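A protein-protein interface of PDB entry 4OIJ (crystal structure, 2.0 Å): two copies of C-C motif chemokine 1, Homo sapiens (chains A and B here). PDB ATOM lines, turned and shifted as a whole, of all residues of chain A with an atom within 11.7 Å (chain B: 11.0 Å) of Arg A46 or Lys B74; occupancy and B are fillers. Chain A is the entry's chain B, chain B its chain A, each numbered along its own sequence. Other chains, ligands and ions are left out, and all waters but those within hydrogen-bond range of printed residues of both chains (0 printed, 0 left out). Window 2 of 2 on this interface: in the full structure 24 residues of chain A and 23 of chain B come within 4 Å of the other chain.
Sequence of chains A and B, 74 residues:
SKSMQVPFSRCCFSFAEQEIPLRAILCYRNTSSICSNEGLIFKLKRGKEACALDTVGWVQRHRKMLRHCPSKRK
The side-chain amino group (NZ) of Lys B72 is in salt-bridge range of the chain-end carboxylate (O) of Lys B74, 3.4 Å away.
The backbone carbonyl oxygen (O) of Ala A50 sits at hydrogen-bond distance from the backbone NH (N) of Phe A42 (2.7 Å).
The side-chain sulfur of Cys A27 is disulfide-bonded to the side-chain sulfur of Cys A69 (2.1 Å).
Ala A24 touches Met B4 (CB to CE, 3.6 Å).
Arg A46 touches Lys B74.
NE2 of Gln B5 touches CE of Lys A48, 3.4 Å away.
Glu A49 touches Gln B5 (O to CB, 3.3 Å).
Pro B7 touches Glu A49 (N to O, 3.9 Å).
Ala A50 touches Met B4 (CB to O, 3.9 Å).
Of chain B, only Lys B74 (3.6 Å) comes within 4 Å of Arg A46.
Of the printed residues of chain B, Lys A48 touches Gln B5.
Printed residues of chain B within 4 Å of Ala A50: Met B4.
Printed residues of chain A within 4 Å of Met B4: Ala A24 (3.6 Å) and Ala A50 (3.9 Å).
Of the printed residues of chain A, Gln B5 touches Lys A48 (3.4 Å) and Glu A49 (3.3 Å).
Pro B70 touches none of the printed residues of chain A.
Lys B72 touches none of the printed residues of chain A.
Of the 15 printed residues of chain A, 5 touch a printed residue of chain B.
Printed residues of chain A that touch a printed residue of chain B: Ala A24, Arg A46, Lys A48, Glu A49 and Ala A50.
Hydrophobic or aromatic side chains of chain A within 4 Å of the printed part of chain B: Ala A24 and Ala A50.
Along chain A the printed residues that touch a printed residue of chain B span positions 24 to 50.
Of the 8 printed residues of chain B, 4 touch a printed residue of chain A.
No position is printed for both chains.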
ATOM      1  N   ARG A  23      27.049  20.443 -26.887  1.00  0.00           N
ATOM      2  CA  ARG A  23      25.810  20.496 -26.072  1.00  0.00           C
ATOM      3  C   ARG A  23      25.602  19.218 -25.218  1.00  0.00           C
ATOM      4  O   ARG A  23      24.897  19.262 -24.225  1.00  0.00           O
ATOM      5  CB  ARG A  23      24.573  20.784 -26.961  1.00  0.00           C
ATOM      6  CG  ARG A  23      24.289  19.708 -28.023  1.00  0.00           C
ATOM      7  CD  ARG A  23      23.306  20.120 -29.128  1.00  0.00           C
ATOM      8  NE  ARG A  23      23.856  19.819 -30.462  1.00  0.00           N
ATOM      9  CZ  ARG A  23      23.863  18.613 -31.036  1.00  0.00           C
ATOM     10  NH1 ARG A  23      24.429  18.439 -32.224  1.00  0.00           N
ATOM     11  NH2 ARG A  23      23.335  17.567 -30.409  1.00  0.00           N
ATOM     12  N   ALA A  24      26.220  18.091 -25.616  1.00  0.00           N
ATOM     13  CA  ALA A  24      26.131  16.802 -24.918  1.00  0.00           C
ATOM     14  C   ALA A  24      27.026  16.719 -23.677  1.00  0.00           C
ATOM     15  O   ALA A  24      26.821  15.827 -22.848  1.00  0.00           O
ATOM     16  CB  ALA A  24      26.485  15.668 -25.879  1.00  0.00           C
ATOM     17  N   ILE A  25      28.019  17.633 -23.558  1.00  0.00           N
ATOM     18  CA  ILE A  25      29.041  17.637 -22.498  1.00  0.00           C
ATOM     19  C   ILE A  25      28.708  18.633 -21.400  1.00  0.00           C
ATOM     20  O   ILE A  25      28.364  19.774 -21.700  1.00  0.00           O
ATOM     21  CB  ILE A  25      30.455  17.932 -23.093  1.00  0.00           C
ATOM     22  CG1 ILE A  25      30.778  17.053 -24.339  1.00  0.00           C
ATOM     23  CG2 ILE A  25      31.550  17.812 -22.033  1.00  0.00           C
ATOM     24  CD1 ILE A  25      31.862  17.621 -25.305  1.00  0.00           C
ATOM     25  N   LEU A  26      28.931  18.225 -20.129  1.00  0.00           N
ATOM     26  CA  LEU A  26      28.716  19.077 -18.966  1.00  0.00           C
ATOM     27  C   LEU A  26      29.971  19.868 -18.644  1.00  0.00           C
ATOM     28  O   LEU A  26      29.899  21.078 -18.429  1.00  0.00           O
ATOM     29  CB  LEU A  26      28.349  18.224 -17.734  1.00  0.00           C
ATOM     30  CG  LEU A  26      26.957  17.617 -17.682  1.00  0.00           C
ATOM     31  CD1 LEU A  26      26.875  16.575 -16.607  1.00  0.00           C
ATOM     32  CD2 LEU A  26      25.895  18.688 -17.432  1.00  0.00           C
ATOM     33  N   CYS A  27      31.128  19.167 -18.597  1.00  0.00           N
ATOM     34  CA  CYS A  27      32.416  19.702 -18.157  1.00  0.00           C
ATOM     35  C   CYS A  27      33.540  18.736 -18.524  1.00  0.00           C
ATOM     36  O   CYS A  27      33.285  17.617 -18.969  1.00  0.00           O
ATOM     37  CB  CYS A  27      32.368  19.946 -16.642  1.00  0.00           C
ATOM     38  SG  CYS A  27      31.849  18.498 -15.663  1.00  0.00           S
ATOM     39  N   PHE A  42      35.745  14.164 -20.958  1.00  0.00           N
ATOM     40  CA  PHE A  42      34.549  14.978 -21.011  1.00  0.00           C
ATOM     41  C   PHE A  42      33.482  14.257 -20.192  1.00  0.00           C
ATOM     42  O   PHE A  42      33.254  13.054 -20.391  1.00  0.00           O
ATOM     43  CB  PHE A  42      34.037  15.146 -22.453  1.00  0.00           C
ATOM     44  CG  PHE A  42      34.916  15.983 -23.349  1.00  0.00           C
ATOM     45  CD1 PHE A  42      35.181  17.318 -23.043  1.00  0.00           C
ATOM     46  CD2 PHE A  42      35.403  15.469 -24.547  1.00  0.00           C
ATOM     47  CE1 PHE A  42      35.940  18.116 -23.911  1.00  0.00           C
ATOM     48  CE2 PHE A  42      36.154  16.272 -25.417  1.00  0.00           C
ATOM     49  CZ  PHE A  42      36.427  17.585 -25.089  1.00  0.00           C
ATOM     50  N   LYS A  43      32.817  14.984 -19.282  1.00  0.00           N
ATOM     51  CA  LYS A  43      31.708  14.435 -18.504  1.00  0.00           C
ATOM     52  C   LYS A  43      30.482  14.681 -19.325  1.00  0.00           C
ATOM     53  O   LYS A  43      30.249  15.810 -19.744  1.00  0.00           O
ATOM     54  CB  LYS A  43      31.564  15.143 -17.146  1.00  0.00           C
ATOM     55  CG  LYS A  43      30.492  14.524 -16.248  1.00  0.00           C
ATOM     56  CD  LYS A  43      30.208  15.336 -14.958  1.00  0.00           C
ATOM     57  CE  LYS A  43      29.389  14.517 -13.977  1.00  0.00           C
ATOM     58  NZ  LYS A  43      28.053  14.099 -14.532  1.00  0.00           N
ATOM     59  N   LEU A  44      29.718  13.638 -19.607  1.00  0.00           N
ATOM     60  CA  LEU A  44      28.500  13.794 -20.396  1.00  0.00           C
ATOM     61  C   LEU A  44      27.303  13.736 -19.432  1.00  0.00           C
ATOM     62  O   LEU A  44      27.481  13.693 -18.209  1.00  0.00           O
ATOM     63  CB  LEU A  44      28.398  12.721 -21.517  1.00  0.00           C
ATOM     64  CG  LEU A  44      29.647  12.459 -22.423  1.00  0.00           C
ATOM     65  CD1 LEU A  44      29.444  11.236 -23.301  1.00  0.00           C
ATOM     66  CD2 LEU A  44      29.966  13.646 -23.313  1.00  0.00           C
ATOM     67  N   LYS A  45      26.096  13.739 -19.970  1.00  0.00           N
ATOM     68  CA  LYS A  45      24.861  13.690 -19.188  1.00  0.00           C
ATOM     69  C   LYS A  45      24.667  12.327 -18.527  1.00  0.00           C
ATOM     70  O   LYS A  45      25.371  11.368 -18.862  1.00  0.00           O
ATOM     71  CB  LYS A  45      23.680  14.064 -20.082  1.00  0.00           C
ATOM     72  CG  LYS A  45      23.357  15.551 -20.027  1.00  0.00           C
ATOM     73  CD  LYS A  45      24.304  16.453 -20.822  1.00  0.00           C
ATOM     74  CE  LYS A  45      23.978  17.912 -20.596  1.00  0.00           C
ATOM     75  NZ  LYS A  45      23.711  18.640 -21.864  1.00  0.00           N
ATOM     76  N   ARG A  46      23.759  12.267 -17.543  1.00  0.00           N
ATOM     77  CA  ARG A  46      23.422  11.066 -16.762  1.00  0.00           C
ATOM     78  C   ARG A  46      24.664  10.248 -16.337  1.00  0.00           C
ATOM     79  O   ARG A  46      24.689   9.019 -16.468  1.00  0.00           O
ATOM     80  CB  ARG A  46      22.336  10.187 -17.454  1.00  0.00           C
ATOM     81  CG  ARG A  46      21.184  10.896 -18.179  1.00  0.00           C
ATOM     82  CD  ARG A  46      20.321  11.802 -17.305  1.00  0.00           C
ATOM     83  NE  ARG A  46      19.043  12.130 -17.941  1.00  0.00           N
ATOM     84  CZ  ARG A  46      18.363  13.254 -17.732  1.00  0.00           C
ATOM     85  NH1 ARG A  46      18.840  14.186 -16.914  1.00  0.00           N
ATOM     86  NH2 ARG A  46      17.209  13.463 -18.353  1.00  0.00           N
ATOM     87  N   GLY A  47      25.694  10.966 -15.881  1.00  0.00           N
ATOM     88  CA  GLY A  47      26.950  10.402 -15.398  1.00  0.00           C
ATOM     89  C   GLY A  47      27.821   9.669 -16.400  1.00  0.00           C
ATOM     90  O   GLY A  47      28.771   8.991 -15.991  1.00  0.00           O
ATOM     91  N   LYS A  48      27.518   9.793 -17.716  1.00  0.00           N
ATOM     92  CA  LYS A  48      28.289   9.149 -18.786  1.00  0.00           C
ATOM     93  C   LYS A  48      29.638   9.871 -18.992  1.00  0.00           C
ATOM     94  O   LYS A  48      29.808  11.016 -18.530  1.00  0.00           O
ATOM     95  CB  LYS A  48      27.489   9.088 -20.084  1.00  0.00           C
ATOM     96  CG  LYS A  48      26.271   8.170 -20.051  1.00  0.00           C
ATOM     97  CD  LYS A  48      25.554   8.155 -21.425  1.00  0.00           C
ATOM     98  CE  LYS A  48      26.231   7.295 -22.475  1.00  0.00           C
ATOM     99  NZ  LYS A  48      25.586   7.421 -23.813  1.00  0.00           N
ATOM    100  N   GLU A  49      30.612   9.184 -19.637  1.00  0.00           N
ATOM    101  CA  GLU A  49      31.950   9.763 -19.847  1.00  0.00           C
ATOM    102  C   GLU A  49      32.699   9.430 -21.152  1.00  0.00           C
ATOM    103  O   GLU A  49      32.491   8.381 -21.792  1.00  0.00           O
ATOM    104  CB  GLU A  49      32.842   9.564 -18.631  1.00  0.00           C
ATOM    105  CG  GLU A  49      33.131  10.852 -17.878  1.00  0.00           C
ATOM    106  CD  GLU A  49      32.812  10.868 -16.399  1.00  0.00           C
ATOM    107  OE1 GLU A  49      32.163   9.911 -15.918  1.00  0.00           O
ATOM    108  OE2 GLU A  49      33.162  11.867 -15.731  1.00  0.00           O
ATOM    109  N   ALA A  50      33.555  10.364 -21.565  1.00  0.00           N
ATOM    110  CA  ALA A  50      34.336  10.153 -22.788  1.00  0.00           C
ATOM    111  C   ALA A  50      35.732  10.727 -22.713  1.00  0.00           C
ATOM    112  O   ALA A  50      35.945  11.931 -22.518  1.00  0.00           O
ATOM    113  CB  ALA A  50      33.605  10.686 -24.003  1.00  0.00           C
ATOM    114  N   CYS A  69      35.299  20.058 -14.394  1.00  0.00           N
ATOM    115  CA  CYS A  69      34.268  19.365 -13.607  1.00  0.00           C
ATOM    116  C   CYS A  69      34.454  19.631 -12.134  1.00  0.00           C
ATOM    117  O   CYS A  69      35.585  19.553 -11.666  1.00  0.00           O
ATOM    118  CB  CYS A  69      34.282  17.863 -13.879  1.00  0.00           C
ATOM    119  SG  CYS A  69      33.549  17.369 -15.452  1.00  0.00           S
ATOM    120  N   MET B   4      28.289   6.778 -27.447  1.00  0.00           N
ATOM    121  CA  MET B   4      29.115   7.987 -27.389  1.00  0.00           C
ATOM    122  C   MET B   4      30.151   7.919 -26.247  1.00  0.00           C
ATOM    123  O   MET B   4      31.047   8.767 -26.175  1.00  0.00           O
ATOM    124  CB  MET B   4      28.219   9.230 -27.243  1.00  0.00           C
ATOM    125  CG  MET B   4      28.876  10.510 -27.718  1.00  0.00           C
ATOM    126  SD  MET B   4      27.724  11.808 -28.242  1.00  0.00           S
ATOM    127  CE  MET B   4      26.887  12.134 -26.677  1.00  0.00           C
ATOM    128  N   GLN B   5      30.038   6.907 -25.371  1.00  0.00           N
ATOM    129  CA  GLN B   5      30.947   6.740 -24.221  1.00  0.00           C
ATOM    130  C   GLN B   5      32.217   5.911 -24.448  1.00  0.00           C
ATOM    131  O   GLN B   5      32.172   4.814 -25.019  1.00  0.00           O
ATOM    132  CB  GLN B   5      30.200   6.316 -22.943  1.00  0.00           C
ATOM    133  CG  GLN B   5      29.508   4.959 -23.005  1.00  0.00           C
ATOM    134  CD  GLN B   5      29.140   4.465 -21.630  1.00  0.00           C
ATOM    135  OE1 GLN B   5      29.996   4.039 -20.844  1.00  0.00           O
ATOM    136  NE2 GLN B   5      27.857   4.496 -21.315  1.00  0.00           N
ATOM    137  N   PRO B   7      34.793   5.258 -21.606  1.00  0.00           N
ATOM    138  CA  PRO B   7      35.086   5.547 -20.196  1.00  0.00           C
ATOM    139  C   PRO B   7      36.543   5.614 -19.841  1.00  0.00           C
ATOM    140  O   PRO B   7      37.339   4.931 -20.460  1.00  0.00           O
ATOM    141  CB  PRO B   7      34.391   4.416 -19.436  1.00  0.00           C
ATOM    142  CG  PRO B   7      33.334   3.923 -20.356  1.00  0.00           C
ATOM    143  CD  PRO B   7      33.884   4.096 -21.739  1.00  0.00           C
ATOM    144  N   PRO B  70      28.445   0.545  -5.447  1.00  0.00           N
ATOM    145  CA  PRO B  70      27.389   0.645  -6.471  1.00  0.00           C
ATOM    146  C   PRO B  70      27.689   1.723  -7.503  1.00  0.00           C
ATOM    147  O   PRO B  70      28.439   2.657  -7.251  1.00  0.00           O
ATOM    148  CB  PRO B  70      26.117   0.953  -5.662  1.00  0.00           C
ATOM    149  CG  PRO B  70      26.611   1.620  -4.431  1.00  0.00           C
ATOM    150  CD  PRO B  70      28.016   1.148  -4.164  1.00  0.00           C
ATOM    151  N   SER B  71      27.063   1.579  -8.662  1.00  0.00           N
ATOM    152  CA  SER B  71      27.152   2.466  -9.809  1.00  0.00           C
ATOM    153  C   SER B  71      25.739   2.877 -10.136  1.00  0.00           C
ATOM    154  O   SER B  71      24.792   2.319  -9.574  1.00  0.00           O
ATOM    155  CB  SER B  71      27.729   1.703 -10.989  1.00  0.00           C
ATOM    156  OG  SER B  71      27.550   2.453 -12.172  1.00  0.00           O
ATOM    157  N   LYS B  72      25.596   3.809 -11.087  1.00  0.00           N
ATOM    158  CA  LYS B  72      24.309   4.303 -11.566  1.00  0.00           C
ATOM    159  C   LYS B  72      24.288   4.309 -13.100  1.00  0.00           C
ATOM    160  O   LYS B  72      25.257   3.883 -13.740  1.00  0.00           O
ATOM    161  CB  LYS B  72      24.042   5.721 -11.010  1.00  0.00           C
ATOM    162  CG  LYS B  72      25.301   6.543 -10.653  1.00  0.00           C
ATOM    163  CD  LYS B  72      25.045   8.050 -10.537  1.00  0.00           C
ATOM    164  CE  LYS B  72      24.111   8.487  -9.432  1.00  0.00           C
ATOM    165  NZ  LYS B  72      23.813   9.940  -9.524  1.00  0.00           N
ATOM    166  N   ARG B  73      23.182   4.779 -13.682  1.00  0.00           N
ATOM    167  CA  ARG B  73      23.003   4.949 -15.116  1.00  0.00           C
ATOM    168  C   ARG B  73      22.054   6.134 -15.358  1.00  0.00           C
ATOM    169  O   ARG B  73      21.271   6.149 -16.330  1.00  0.00           O
ATOM    170  CB  ARG B  73      22.549   3.645 -15.795  1.00  0.00           C
ATOM    171  CG  ARG B  73      23.239   3.417 -17.138  1.00  0.00           C
ATOM    172  CD  ARG B  73      24.178   2.217 -17.124  1.00  0.00           C
ATOM    173  NE  ARG B  73      23.432   0.970 -17.291  1.00  0.00           N
ATOM    174  CZ  ARG B  73      23.974  -0.230 -17.474  1.00  0.00           C
ATOM    175  NH1 ARG B  73      25.296  -0.373 -17.525  1.00  0.00           N
ATOM    176  NH2 ARG B  73      23.202  -1.297 -17.614  1.00  0.00           N
ATOM    177  N   LYS B  74      22.138   7.134 -14.440  1.00  0.00           N
ATOM    178  CA  LYS B  74      21.368   8.391 -14.441  1.00  0.00           C
ATOM    179  C   LYS B  74      21.943   9.436 -13.462  1.00  0.00           C
ATOM    180  O   LYS B  74      22.878   9.110 -12.696  1.00  0.00           O
ATOM    181  CB  LYS B  74      19.865   8.152 -14.175  1.00  0.00           C
ATOM    182  OXT LYS B  74      21.459  10.591 -13.470  1.00  0.00           O
